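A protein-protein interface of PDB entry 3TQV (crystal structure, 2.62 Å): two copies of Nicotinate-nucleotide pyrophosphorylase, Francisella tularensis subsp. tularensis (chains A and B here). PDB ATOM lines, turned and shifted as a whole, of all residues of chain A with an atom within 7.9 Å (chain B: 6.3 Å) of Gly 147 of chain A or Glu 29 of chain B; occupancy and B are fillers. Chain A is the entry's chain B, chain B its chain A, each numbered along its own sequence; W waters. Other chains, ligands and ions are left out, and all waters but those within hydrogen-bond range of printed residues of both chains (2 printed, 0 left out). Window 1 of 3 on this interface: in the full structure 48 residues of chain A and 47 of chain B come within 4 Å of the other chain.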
ATOM      1  N   VAL A  14      24.138  23.032  14.844  1.00  0.00           N
ATOM      2  CA  VAL A  14      23.235  22.084  15.484  1.00  0.00           C
ATOM      3  C   VAL A  14      22.469  22.796  16.582  1.00  0.00           C
ATOM      4  O   VAL A  14      23.062  23.516  17.380  1.00  0.00           O
ATOM      5  CB  VAL A  14      24.003  20.898  16.100  1.00  0.00           C
ATOM      6  CG1 VAL A  14      23.038  19.901  16.776  1.00  0.00           C
ATOM      7  CG2 VAL A  14      24.853  20.218  15.036  1.00  0.00           C
ATOM      8  N   ILE A  18      19.446  20.125  21.105  1.00  0.00           N
ATOM      9  CA  ILE A  18      19.957  18.835  20.654  1.00  0.00           C
ATOM     10  C   ILE A  18      21.407  18.594  21.117  1.00  0.00           C
ATOM     11  O   ILE A  18      21.788  17.479  21.453  1.00  0.00           O
ATOM     12  CB  ILE A  18      19.888  18.713  19.120  1.00  0.00           C
ATOM     13  CG1 ILE A  18      18.444  18.733  18.636  1.00  0.00           C
ATOM     14  CG2 ILE A  18      20.569  17.437  18.644  1.00  0.00           C
ATOM     15  CD1 ILE A  18      17.695  17.447  18.914  1.00  0.00           C
ATOM     16  N   ARG A  21      21.003  17.809  25.012  1.00  0.00           N
ATOM     17  CA  ARG A  21      20.445  16.506  25.362  1.00  0.00           C
ATOM     18  C   ARG A  21      21.413  15.365  25.073  1.00  0.00           C
ATOM     19  O   ARG A  21      21.505  14.402  25.831  1.00  0.00           O
ATOM     20  CB  ARG A  21      19.143  16.265  24.610  1.00  0.00           C
ATOM     21  CG  ARG A  21      18.475  14.975  24.979  1.00  0.00           C
ATOM     22  CD  ARG A  21      17.951  14.306  23.740  1.00  0.00           C
ATOM     23  NE  ARG A  21      16.968  15.142  23.060  1.00  0.00           N
ATOM     24  CZ  ARG A  21      16.644  15.013  21.775  1.00  0.00           C
ATOM     25  NH1 ARG A  21      17.242  14.096  21.026  1.00  0.00           N
ATOM     26  NH2 ARG A  21      15.738  15.817  21.236  1.00  0.00           N
ATOM     27  N   LEU A  22      22.120  15.479  23.959  1.00  0.00           N
ATOM     28  CA  LEU A  22      23.106  14.493  23.570  1.00  0.00           C
ATOM     29  C   LEU A  22      24.297  14.449  24.541  1.00  0.00           C
ATOM     30  O   LEU A  22      24.859  13.392  24.807  1.00  0.00           O
ATOM     31  CB  LEU A  22      23.587  14.790  22.153  1.00  0.00           C
ATOM     32  CG  LEU A  22      22.920  13.986  21.040  1.00  0.00           C
ATOM     33  CD1 LEU A  22      23.311  14.526  19.672  1.00  0.00           C
ATOM     34  CD2 LEU A  22      23.276  12.510  21.170  1.00  0.00           C
ATOM     35  N   GLU A  25      22.872  12.947  28.189  1.00  0.00           N
ATOM     36  CA  GLU A  25      22.786  11.492  28.103  1.00  0.00           C
ATOM     37  C   GLU A  25      24.165  10.789  28.006  1.00  0.00           C
ATOM     38  O   GLU A  25      24.350   9.691  28.531  1.00  0.00           O
ATOM     39  CB  GLU A  25      21.887  11.092  26.927  1.00  0.00           C
ATOM     40  CG  GLU A  25      20.408  11.329  27.167  1.00  0.00           C
ATOM     41  CD  GLU A  25      19.598  11.357  25.870  1.00  0.00           C
ATOM     42  OE1 GLU A  25      20.146  10.962  24.815  1.00  0.00           O
ATOM     43  OE2 GLU A  25      18.417  11.790  25.899  1.00  0.00           O
ATOM     44  N   PHE A  63      29.690  20.750  21.182  1.00  0.00           N
ATOM     45  CA  PHE A  63      29.535  19.654  22.139  1.00  0.00           C
ATOM     46  C   PHE A  63      30.551  19.725  23.275  1.00  0.00           C
ATOM     47  O   PHE A  63      30.185  19.753  24.450  1.00  0.00           O
ATOM     48  CB  PHE A  63      29.601  18.289  21.430  1.00  0.00           C
ATOM     49  CG  PHE A  63      28.474  18.063  20.456  1.00  0.00           C
ATOM     50  CD1 PHE A  63      27.301  17.459  20.868  1.00  0.00           C
ATOM     51  CD2 PHE A  63      28.581  18.481  19.138  1.00  0.00           C
ATOM     52  CE1 PHE A  63      26.253  17.259  19.992  1.00  0.00           C
ATOM     53  CE2 PHE A  63      27.537  18.275  18.250  1.00  0.00           C
ATOM     54  CZ  PHE A  63      26.368  17.660  18.685  1.00  0.00           C
ATOM     55  N   PHE A 113      33.180  13.026  21.240  1.00  0.00           N
ATOM     56  CA  PHE A 113      32.415  13.825  20.290  1.00  0.00           C
ATOM     57  C   PHE A 113      33.276  14.379  19.152  1.00  0.00           C
ATOM     58  O   PHE A 113      32.864  14.373  17.987  1.00  0.00           O
ATOM     59  CB  PHE A 113      31.663  14.954  20.984  1.00  0.00           C
ATOM     60  CG  PHE A 113      30.344  14.538  21.565  1.00  0.00           C
ATOM     61  CD1 PHE A 113      30.216  14.302  22.918  1.00  0.00           C
ATOM     62  CD2 PHE A 113      29.231  14.405  20.758  1.00  0.00           C
ATOM     63  CE1 PHE A 113      29.012  13.952  23.454  1.00  0.00           C
ATOM     64  CE2 PHE A 113      28.013  14.053  21.297  1.00  0.00           C
ATOM     65  CZ  PHE A 113      27.901  13.822  22.643  1.00  0.00           C
ATOM     66  N   MET A 116      34.419  11.621  16.633  1.00  0.00           N
ATOM     67  CA  MET A 116      33.360  11.131  15.799  1.00  0.00           C
ATOM     68  C   MET A 116      33.037  12.135  14.709  1.00  0.00           C
ATOM     69  O   MET A 116      33.155  11.837  13.516  1.00  0.00           O
ATOM     70  CB  MET A 116      32.135  10.877  16.658  1.00  0.00           C
ATOM     71  CG  MET A 116      31.032  10.176  15.924  1.00  0.00           C
ATOM     72  SD  MET A 116      29.351  10.491  16.807  1.00  0.00           S
ATOM     73  CE  MET A 116      28.175   9.925  15.361  1.00  0.00           C
ATOM     74  N   ARG A 142      20.140   9.838   4.463  1.00  0.00           N
ATOM     75  CA  ARG A 142      19.591   9.567   5.794  1.00  0.00           C
ATOM     76  C   ARG A 142      20.321   8.396   6.487  1.00  0.00           C
ATOM     77  O   ARG A 142      19.955   8.000   7.606  1.00  0.00           O
ATOM     78  CB  ARG A 142      18.068   9.335   5.733  1.00  0.00           C
ATOM     79  CG  ARG A 142      17.259  10.625   5.451  1.00  0.00           C
ATOM     80  CD  ARG A 142      15.819  10.380   4.958  1.00  0.00           C
ATOM     81  NE  ARG A 142      15.035   9.522   5.847  1.00  0.00           N
ATOM     82  CZ  ARG A 142      14.584   8.301   5.526  1.00  0.00           C
ATOM     83  NH1 ARG A 142      14.837   7.787   4.333  1.00  0.00           N
ATOM     84  NH2 ARG A 142      13.867   7.589   6.395  1.00  0.00           N
ATOM     85  N   THR A 144      22.438   7.532   8.682  1.00  0.00           N
ATOM     86  CA  THR A 144      22.997   8.294   9.767  1.00  0.00           C
ATOM     87  C   THR A 144      23.056   7.443  11.053  1.00  0.00           C
ATOM     88  O   THR A 144      22.327   6.447  11.176  1.00  0.00           O
ATOM     89  CB  THR A 144      22.067   9.487   9.974  1.00  0.00           C
ATOM     90  OG1 THR A 144      22.706  10.684   9.523  1.00  0.00           O
ATOM     91  CG2 THR A 144      21.639   9.616  11.425  1.00  0.00           C
ATOM     92  N   ILE A 145      23.915   7.820  12.003  1.00  0.00           N
ATOM     93  CA  ILE A 145      23.871   7.204  13.333  1.00  0.00           C
ATOM     94  C   ILE A 145      22.665   7.719  14.124  1.00  0.00           C
ATOM     95  O   ILE A 145      22.502   8.921  14.301  1.00  0.00           O
ATOM     96  CB  ILE A 145      25.128   7.475  14.171  1.00  0.00           C
ATOM     97  CG1 ILE A 145      26.387   7.265  13.330  1.00  0.00           C
ATOM     98  CG2 ILE A 145      25.114   6.563  15.412  1.00  0.00           C
ATOM     99  CD1 ILE A 145      26.415   5.912  12.610  1.00  0.00           C
ATOM    100  N   PRO A 146      21.816   6.807  14.601  1.00  0.00           N
ATOM    101  CA  PRO A 146      20.594   7.277  15.242  1.00  0.00           C
ATOM    102  C   PRO A 146      20.870   8.342  16.305  1.00  0.00           C
ATOM    103  O   PRO A 146      21.797   8.189  17.105  1.00  0.00           O
ATOM    104  CB  PRO A 146      20.033   5.996  15.853  1.00  0.00           C
ATOM    105  CG  PRO A 146      20.404   4.948  14.838  1.00  0.00           C
ATOM    106  CD  PRO A 146      21.807   5.347  14.421  1.00  0.00           C
ATOM    107  N   GLY A 147      20.074   9.411  16.288  1.00  0.00           N
ATOM    108  CA  GLY A 147      20.172  10.479  17.261  1.00  0.00           C
ATOM    109  C   GLY A 147      21.158  11.546  16.841  1.00  0.00           C
ATOM    110  O   GLY A 147      21.293  12.573  17.499  1.00  0.00           O
ATOM    111  N   PHE A 148      21.862  11.283  15.751  1.00  0.00           N
ATOM    112  CA  PHE A 148      22.936  12.141  15.272  1.00  0.00           C
ATOM    113  C   PHE A 148      22.638  12.586  13.861  1.00  0.00           C
ATOM    114  O   PHE A 148      23.562  12.788  13.074  1.00  0.00           O
ATOM    115  CB  PHE A 148      24.271  11.391  15.271  1.00  0.00           C
ATOM    116  CG  PHE A 148      24.882  11.244  16.626  1.00  0.00           C
ATOM    117  CD1 PHE A 148      25.887  12.109  17.038  1.00  0.00           C
ATOM    118  CD2 PHE A 148      24.450  10.239  17.486  1.00  0.00           C
ATOM    119  CE1 PHE A 148      26.453  12.006  18.301  1.00  0.00           C
ATOM    120  CE2 PHE A 148      25.013  10.097  18.753  1.00  0.00           C
ATOM    121  CZ  PHE A 148      26.033  10.991  19.170  1.00  0.00           C
ATOM    122  N   ARG A 149      21.353  12.721  13.543  1.00  0.00           N
ATOM    123  CA  ARG A 149      20.949  13.170  12.217  1.00  0.00           C
ATOM    124  C   ARG A 149      21.508  14.555  11.923  1.00  0.00           C
ATOM    125  O   ARG A 149      22.263  14.743  10.971  1.00  0.00           O
ATOM    126  CB  ARG A 149      19.426  13.185  12.097  1.00  0.00           C
ATOM    127  CG  ARG A 149      18.908  14.048  10.968  1.00  0.00           C
ATOM    128  CD  ARG A 149      19.030  13.406   9.599  1.00  0.00           C
ATOM    129  NE  ARG A 149      18.115  12.276   9.483  1.00  0.00           N
ATOM    130  CZ  ARG A 149      18.528  11.044   9.241  1.00  0.00           C
ATOM    131  NH1 ARG A 149      19.824  10.819   9.076  1.00  0.00           N
ATOM    132  NH2 ARG A 149      17.666  10.048   9.159  1.00  0.00           N
ATOM    133  N   LEU A 150      21.144  15.520  12.761  1.00  0.00           N
ATOM    134  CA  LEU A 150      21.584  16.890  12.565  1.00  0.00           C
ATOM    135  C   LEU A 150      23.093  17.048  12.806  1.00  0.00           C
ATOM    136  O   LEU A 150      23.793  17.735  12.055  1.00  0.00           O
ATOM    137  CB  LEU A 150      20.763  17.840  13.446  1.00  0.00           C
ATOM    138  CG  LEU A 150      19.317  18.042  12.969  1.00  0.00           C
ATOM    139  CD1 LEU A 150      18.540  18.894  13.961  1.00  0.00           C
ATOM    140  CD2 LEU A 150      19.252  18.660  11.565  1.00  0.00           C
ATOM    141  N   ALA A 151      23.584  16.387  13.848  1.00  0.00           N
ATOM    142  CA  ALA A 151      25.006  16.407  14.176  1.00  0.00           C
ATOM    143  C   ALA A 151      25.855  15.993  12.981  1.00  0.00           C
ATOM    144  O   ALA A 151      26.870  16.630  12.693  1.00  0.00           O
ATOM    145  CB  ALA A 151      25.294  15.504  15.391  1.00  0.00           C
ATOM    146  N   GLN A 152      25.439  14.934  12.279  1.00  0.00           N
ATOM    147  CA  GLN A 152      26.154  14.485  11.079  1.00  0.00           C
ATOM    148  C   GLN A 152      25.926  15.356   9.812  1.00  0.00           C
ATOM    149  O   GLN A 152      26.808  15.491   8.975  1.00  0.00           O
ATOM    150  CB  GLN A 152      25.872  13.003  10.801  1.00  0.00           C
ATOM    151  CG  GLN A 152      26.459  12.075  11.866  1.00  0.00           C
ATOM    152  CD  GLN A 152      26.803  10.682  11.331  1.00  0.00           C
ATOM    153  OE1 GLN A 152      27.975  10.370  11.054  1.00  0.00           O
ATOM    154  NE2 GLN A 152      25.783   9.841  11.181  1.00  0.00           N
ATOM    155  N   ILE A 166      16.877  16.752   5.067  1.00  0.00           N
ATOM    156  CA  ILE A 166      17.095  16.335   6.447  1.00  0.00           C
ATOM    157  C   ILE A 166      16.347  15.049   6.810  1.00  0.00           C
ATOM    158  O   ILE A 166      16.882  14.210   7.535  1.00  0.00           O
ATOM    159  CB  ILE A 166      16.717  17.433   7.471  1.00  0.00           C
ATOM    160  CG1 ILE A 166      17.404  18.751   7.117  1.00  0.00           C
ATOM    161  CG2 ILE A 166      17.039  16.969   8.904  1.00  0.00           C
ATOM    162  CD1 ILE A 166      18.886  18.595   6.775  1.00  0.00           C
ATOM    163  N   GLY A 167      15.119  14.890   6.322  1.00  0.00           N
ATOM    164  CA  GLY A 167      14.310  13.754   6.730  1.00  0.00           C
ATOM    165  C   GLY A 167      13.141  13.355   5.854  1.00  0.00           C
ATOM    166  O   GLY A 167      13.224  13.423   4.623  1.00  0.00           O
ATOM    167  N   LEU A 168      12.050  12.913   6.480  1.00  0.00           N
ATOM    168  CA  LEU A 168      10.873  12.498   5.719  1.00  0.00           C
ATOM    169  C   LEU A 168       9.863  13.643   5.548  1.00  0.00           C
ATOM    170  O   LEU A 168       8.859  13.506   4.844  1.00  0.00           O
ATOM    171  CB  LEU A 168      10.211  11.269   6.359  1.00  0.00           C
ATOM    172  CG  LEU A 168      11.044   9.976   6.440  1.00  0.00           C
ATOM    173  CD1 LEU A 168      10.478   8.994   7.470  1.00  0.00           C
ATOM    174  CD2 LEU A 168      11.222   9.293   5.077  1.00  0.00           C
ATOM    175  N   PHE A 169      10.155  14.784   6.169  1.00  0.00           N
ATOM    176  CA  PHE A 169       9.204  15.890   6.229  1.00  0.00           C
ATOM    177  C   PHE A 169       9.546  17.093   5.329  1.00  0.00           C
ATOM    178  O   PHE A 169       8.656  17.706   4.749  1.00  0.00           O
ATOM    179  CB  PHE A 169       9.060  16.353   7.677  1.00  0.00           C
ATOM    180  CG  PHE A 169      10.358  16.738   8.305  1.00  0.00           C
ATOM    181  CD1 PHE A 169      10.873  18.013   8.129  1.00  0.00           C
ATOM    182  CD2 PHE A 169      11.077  15.821   9.048  1.00  0.00           C
ATOM    183  CE1 PHE A 169      12.073  18.366   8.690  1.00  0.00           C
ATOM    184  CE2 PHE A 169      12.281  16.160   9.624  1.00  0.00           C
ATOM    185  CZ  PHE A 169      12.783  17.435   9.446  1.00  0.00           C
ATOM    186  N   ASP A 170      10.821  17.441   5.216  1.00  0.00           N
ATOM    187  CA  ASP A 170      11.197  18.653   4.483  1.00  0.00           C
ATOM    188  C   ASP A 170      11.225  18.499   2.954  1.00  0.00           C
ATOM    189  O   ASP A 170      11.296  19.492   2.222  1.00  0.00           O
ATOM    190  CB  ASP A 170      12.535  19.228   5.000  1.00  0.00           C
ATOM    191  CG  ASP A 170      13.659  18.177   5.087  1.00  0.00           C
ATOM    192  OD1 ASP A 170      13.379  16.961   5.057  1.00  0.00           O
ATOM    193  OD2 ASP A 170      14.831  18.583   5.211  1.00  0.00           O
ATOM    194  N   LEU B  22      16.349   5.929  22.828  1.00  0.00           N
ATOM    195  CA  LEU B  22      17.094   6.015  21.583  1.00  0.00           C
ATOM    196  C   LEU B  22      16.159   5.986  20.375  1.00  0.00           C
ATOM    197  O   LEU B  22      16.165   6.906  19.558  1.00  0.00           O
ATOM    198  CB  LEU B  22      18.140   4.908  21.494  1.00  0.00           C
ATOM    199  CG  LEU B  22      19.533   5.261  22.039  1.00  0.00           C
ATOM    200  CD1 LEU B  22      20.470   4.036  22.079  1.00  0.00           C
ATOM    201  CD2 LEU B  22      20.165   6.385  21.231  1.00  0.00           C
ATOM    202  N   ARG B  24      12.909   6.456  20.172  1.00  0.00           N
ATOM    203  CA  ARG B  24      12.080   7.661  20.164  1.00  0.00           C
ATOM    204  C   ARG B  24      12.765   8.894  19.524  1.00  0.00           C
ATOM    205  O   ARG B  24      12.210   9.537  18.624  1.00  0.00           O
ATOM    206  CB  ARG B  24      11.628   7.996  21.574  1.00  0.00           C
ATOM    207  CG  ARG B  24      10.524   9.012  21.624  1.00  0.00           C
ATOM    208  CD  ARG B  24      10.431   9.702  22.990  1.00  0.00           C
ATOM    209  NE  ARG B  24      10.123   8.761  24.060  1.00  0.00           N
ATOM    210  CZ  ARG B  24      10.902   8.547  25.117  1.00  0.00           C
ATOM    211  NH1 ARG B  24      12.039   9.217  25.262  1.00  0.00           N
ATOM    212  NH2 ARG B  24      10.539   7.659  26.036  1.00  0.00           N
ATOM    213  N   GLU B  25      13.963   9.235  19.983  1.00  0.00           N
ATOM    214  CA  GLU B  25      14.654  10.406  19.448  1.00  0.00           C
ATOM    215  C   GLU B  25      15.040  10.266  17.966  1.00  0.00           C
ATOM    216  O   GLU B  25      15.034  11.244  17.217  1.00  0.00           O
ATOM    217  CB  GLU B  25      15.863  10.758  20.321  1.00  0.00           C
ATOM    218  CG  GLU B  25      15.484  11.502  21.606  1.00  0.00           C
ATOM    219  CD  GLU B  25      16.396  11.173  22.782  1.00  0.00           C
ATOM    220  OE1 GLU B  25      17.448  10.526  22.579  1.00  0.00           O
ATOM    221  OE2 GLU B  25      16.059  11.552  23.922  1.00  0.00           O
ATOM    222  N   SER B  26      15.357   9.047  17.542  1.00  0.00           N
ATOM    223  CA  SER B  26      15.783   8.809  16.168  1.00  0.00           C
ATOM    224  C   SER B  26      14.605   8.815  15.219  1.00  0.00           C
ATOM    225  O   SER B  26      14.744   9.199  14.055  1.00  0.00           O
ATOM    226  CB  SER B  26      16.569   7.502  16.040  1.00  0.00           C
ATOM    227  OG  SER B  26      16.012   6.485  16.845  1.00  0.00           O
ATOM    228  N   LEU B  27      13.446   8.381  15.712  1.00  0.00           N
ATOM    229  CA  LEU B  27      12.199   8.509  14.953  1.00  0.00           C
ATOM    230  C   LEU B  27      11.835   9.997  14.841  1.00  0.00           C
ATOM    231  O   LEU B  27      11.561  10.515  13.751  1.00  0.00           O
ATOM    232  CB  LEU B  27      11.071   7.722  15.622  1.00  0.00           C
ATOM    233  CG  LEU B  27      11.230   6.194  15.704  1.00  0.00           C
ATOM    234  CD1 LEU B  27      10.132   5.565  16.550  1.00  0.00           C
ATOM    235  CD2 LEU B  27      11.270   5.541  14.329  1.00  0.00           C
ATOM    236  N   ALA B  28      11.863  10.692  15.971  1.00  0.00           N
ATOM    237  CA  ALA B  28      11.526  12.106  15.982  1.00  0.00           C
ATOM    238  C   ALA B  28      12.382  12.880  14.980  1.00  0.00           C
ATOM    239  O   ALA B  28      11.867  13.659  14.173  1.00  0.00           O
ATOM    240  CB  ALA B  28      11.681  12.676  17.377  1.00  0.00           C
ATOM    241  N   GLU B  29      13.687  12.657  15.027  1.00  0.00           N
ATOM    242  CA  GLU B  29      14.614  13.403  14.201  1.00  0.00           C
ATOM    243  C   GLU B  29      14.394  13.110  12.723  1.00  0.00           C
ATOM    244  O   GLU B  29      14.771  13.914  11.863  1.00  0.00           O
ATOM    245  CB  GLU B  29      16.057  13.059  14.577  1.00  0.00           C
ATOM    246  CG  GLU B  29      16.552  11.750  13.960  1.00  0.00           C
ATOM    247  CD  GLU B  29      17.940  11.374  14.410  1.00  0.00           C
ATOM    248  OE1 GLU B  29      18.348  10.234  14.138  1.00  0.00           O
ATOM    249  OE2 GLU B  29      18.627  12.212  15.032  1.00  0.00           O
ATOM    250  N   ASP B  30      13.811  11.958  12.408  1.00  0.00           N
ATOM    251  CA  ASP B  30      13.586  11.625  11.000  1.00  0.00           C
ATOM    252  C   ASP B  30      12.155  12.008  10.538  1.00  0.00           C
ATOM    253  O   ASP B  30      11.954  12.461   9.402  1.00  0.00           O
ATOM    254  CB  ASP B  30      13.907  10.131  10.732  1.00  0.00           C
ATOM    255  CG  ASP B  30      13.981   9.785   9.223  1.00  0.00           C
ATOM    256  OD1 ASP B  30      14.586  10.552   8.425  1.00  0.00           O
ATOM    257  OD2 ASP B  30      13.424   8.734   8.831  1.00  0.00           O
ATOM    258  N   ILE B  31      11.187  11.843  11.436  1.00  0.00           N
ATOM    259  CA  ILE B  31       9.780  11.842  11.060  1.00  0.00           C
ATOM    260  C   ILE B  31       9.158  13.235  11.201  1.00  0.00           C
ATOM    261  O   ILE B  31       8.418  13.686  10.313  1.00  0.00           O
ATOM    262  CB  ILE B  31       8.952  10.829  11.918  1.00  0.00           C
ATOM    263  CG1 ILE B  31       8.859   9.440  11.273  1.00  0.00           C
ATOM    264  CG2 ILE B  31       7.529  11.332  12.117  1.00  0.00           C
ATOM    265  CD1 ILE B  31      10.149   8.851  10.849  1.00  0.00           C
ATOM    266  N   ALA B  32       9.447  13.903  12.321  1.00  0.00           N
ATOM    267  CA  ALA B  32       8.809  15.175  12.653  1.00  0.00           C
ATOM    268  C   ALA B  32       7.294  15.109  12.450  1.00  0.00           C
ATOM    269  O   ALA B  32       6.661  14.123  12.820  1.00  0.00           O
ATOM    270  CB  ALA B  32       9.422  16.326  11.852  1.00  0.00           C
ATOM    271  N   PHE B 113      19.849   1.245  12.634  1.00  0.00           N
ATOM    272  CA  PHE B 113      20.288   0.549  13.850  1.00  0.00           C
ATOM    273  C   PHE B 113      21.079  -0.753  13.586  1.00  0.00           C
ATOM    274  O   PHE B 113      22.189  -0.931  14.105  1.00  0.00           O
ATOM    275  CB  PHE B 113      19.128   0.308  14.829  1.00  0.00           C
ATOM    276  CG  PHE B 113      18.842   1.476  15.744  1.00  0.00           C
ATOM    277  CD1 PHE B 113      17.712   2.262  15.560  1.00  0.00           C
ATOM    278  CD2 PHE B 113      19.702   1.787  16.788  1.00  0.00           C
ATOM    279  CE1 PHE B 113      17.441   3.323  16.401  1.00  0.00           C
ATOM    280  CE2 PHE B 113      19.431   2.857  17.636  1.00  0.00           C
ATOM    281  CZ  PHE B 113      18.306   3.630  17.434  1.00  0.00           C
ATOM    282  N   PHE B 148      25.586   5.482  22.992  1.00  0.00           N
ATOM    283  CA  PHE B 148      25.581   4.059  22.653  1.00  0.00           C
ATOM    284  C   PHE B 148      26.575   3.265  23.480  1.00  0.00           C
ATOM    285  O   PHE B 148      27.120   2.269  23.004  1.00  0.00           O
ATOM    286  CB  PHE B 148      25.903   3.844  21.177  1.00  0.00           C
ATOM    287  CG  PHE B 148      24.856   4.363  20.246  1.00  0.00           C
ATOM    288  CD1 PHE B 148      23.955   3.498  19.651  1.00  0.00           C
ATOM    289  CD2 PHE B 148      24.785   5.713  19.949  1.00  0.00           C
ATOM    290  CE1 PHE B 148      22.984   3.960  18.777  1.00  0.00           C
ATOM    291  CE2 PHE B 148      23.828   6.189  19.078  1.00  0.00           C
ATOM    292  CZ  PHE B 148      22.917   5.307  18.486  1.00  0.00           C
HETATM  293  O   HOH W   1      15.965   7.408   9.203  1.00  0.00           O
HETATM  294  O   HOH W   2      19.111  15.330  15.132  1.00  0.00           O
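CG2 of Ile 145 of chain A touches CE2 of Phe 148 of chain B (3.9 Å).
Ser 26 of chain B touches Pro 146 of chain A (CB to CB, 3.8 Å).
Pro 146 of chain A touches Glu 29 of chain B.
Pro 146 of chain A touches Phe 113 of chain B.
Pro 146 of chain A touches Phe 148 of chain B (O to CZ, 3.4 Å).
Ser 26 of chain B touches Gly 147 of chain A.
Asp 30 of chain B touches Gly 167 of chain A (OD1 to CA, 3.6 Å).
Leu 168 of chain A touches Ile 31 of chain B (CD1 to CD1, 3.4 Å).
Phe 169 of chain A touches Asp 30 of chain B.
Ala 32 of chain B touches Phe 169 of chain A.
Water W1 lies within hydrogen-bond range of the side-chain carboxylate of Asp 30 of chain B (2.9 Å) and the guanidinium group of Arg 149 of chain A (3.1 Å).
Water W2 lies within hydrogen-bond range of the backbone NH (N) of Leu 150 of chain A (3.1 Å) and the side-chain carboxylate (OE2) of Glu 29 of chain B (3.2 Å).
OG of Ser 26 of chain B sits at hydrogen-bond distance from O of Leu 22 of chain B, at 2.7 Å.
NH1 of Arg 149 of chain A lies within hydrogen-bond range of O of Arg 142 of chain A, at 3.2 Å.
The side-chain hydroxyl of Thr 144 of chain A sits close to the guanidinium group of Arg 149 of chain A (2.9 Å).
NE2 of Gln 152 of chain A sits close to N of Ile 145 of chain A, at 2.9 Å.
The backbone carbonyl oxygen (O) of Ile 166 of chain A sits at hydrogen-bond distance from the guanidinium group (NE) of Arg 149 of chain A, 3.0 Å away.
The backbone NH (N) of Gly 167 of chain A lies within hydrogen-bond range of the side-chain carboxylate (OD1) of Asp 170 of chain A (3.0 Å).
Glu 25 of chain A touches its own counterpart, Glu 25 of chain B.
Of the 19 pairs that touch across the chains among the printed residues, 1 has its exchanged pair printed and touching as well.
Of the 23 printed residues of chain A, 11 touch a printed residue of chain B.
Printed residues of chain A that touch a printed residue of chain B: Arg 21, Glu 25, Arg 142, Ile 145, Pro 146, Gly 147, Phe 148, Arg 149, Gly 167, Leu 168 and Phe 169.
Printed residues of chain B that touch a printed residue of chain A: Glu 25, Ser 26, Glu 29, Asp 30, Ile 31, Ala 32, Phe 113 and Phe 148.
Among the printed residues, 19 pairs touch across the chains.
Among the printed residues, Asp or Glu carboxylates within 4 Å of a Lys or Arg side-chain nitrogen of the other chain: Arg 21 of chain A with Glu 25 of chain B, Arg 142 of chain A with Asp 30 of chain B and Arg 149 of chain A with Asp 30 of chain B.
Of chain A, only Pro 146, Gly 147, Phe 148 and Arg 149 come within 4 Å of Glu 29 of chain B.
No residue of chain A comes within 4 Å of Ala 28 of chain B.
Printed residues of chain B within 4 Å of Arg 21 of chain A: Glu 25 (3.2 Å).
Of the printed residues of chain B, Gly 167 of chain A touches Asp 30.
Ile 18 of chain A touches none of the printed residues of chain B.
Phe 63 of chain A touches none of the printed residues of chain B.
NE of Arg 21 of chain A lies within salt-bridge range of OE2 of Glu 25 of chain B (3.8 Å).
The side-chain carboxylate (OE1) of Glu 29 of chain B lies within hydrogen-bond range of the backbone NH (N) of Gly 147 of chain A, at 2.9 Å.
The side-chain carboxylate (OE2) of Glu 29 of chain B sits at hydrogen-bond distance from the backbone NH (N) of Phe 148 of chain A, 3.4 Å away.
The backbone NH of Arg 149 of chain A is in hydrogen-bond range of the side-chain carboxylate of Glu 29 of chain B, at 3.1 Å.
The guanidinium group (NH2) of Arg 142 of chain A is in salt-bridge range of the side-chain carboxylate (OD2) of Asp 30 of chain B.
The side-chain carboxylate (OD1) of Asp 30 of chain B is in salt-bridge range of the guanidinium group (NH2) of Arg 149 of chain A, 3.2 Å away.
O of Asp 30 of chain B lies within hydrogen-bond range of N of Leu 168 of chain A.
The side-chain carboxylate (OE2) of Glu 25 of chain B lies close to the side-chain carboxylate (OE2) of Glu 25 of chain A, 3.1 Å away.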
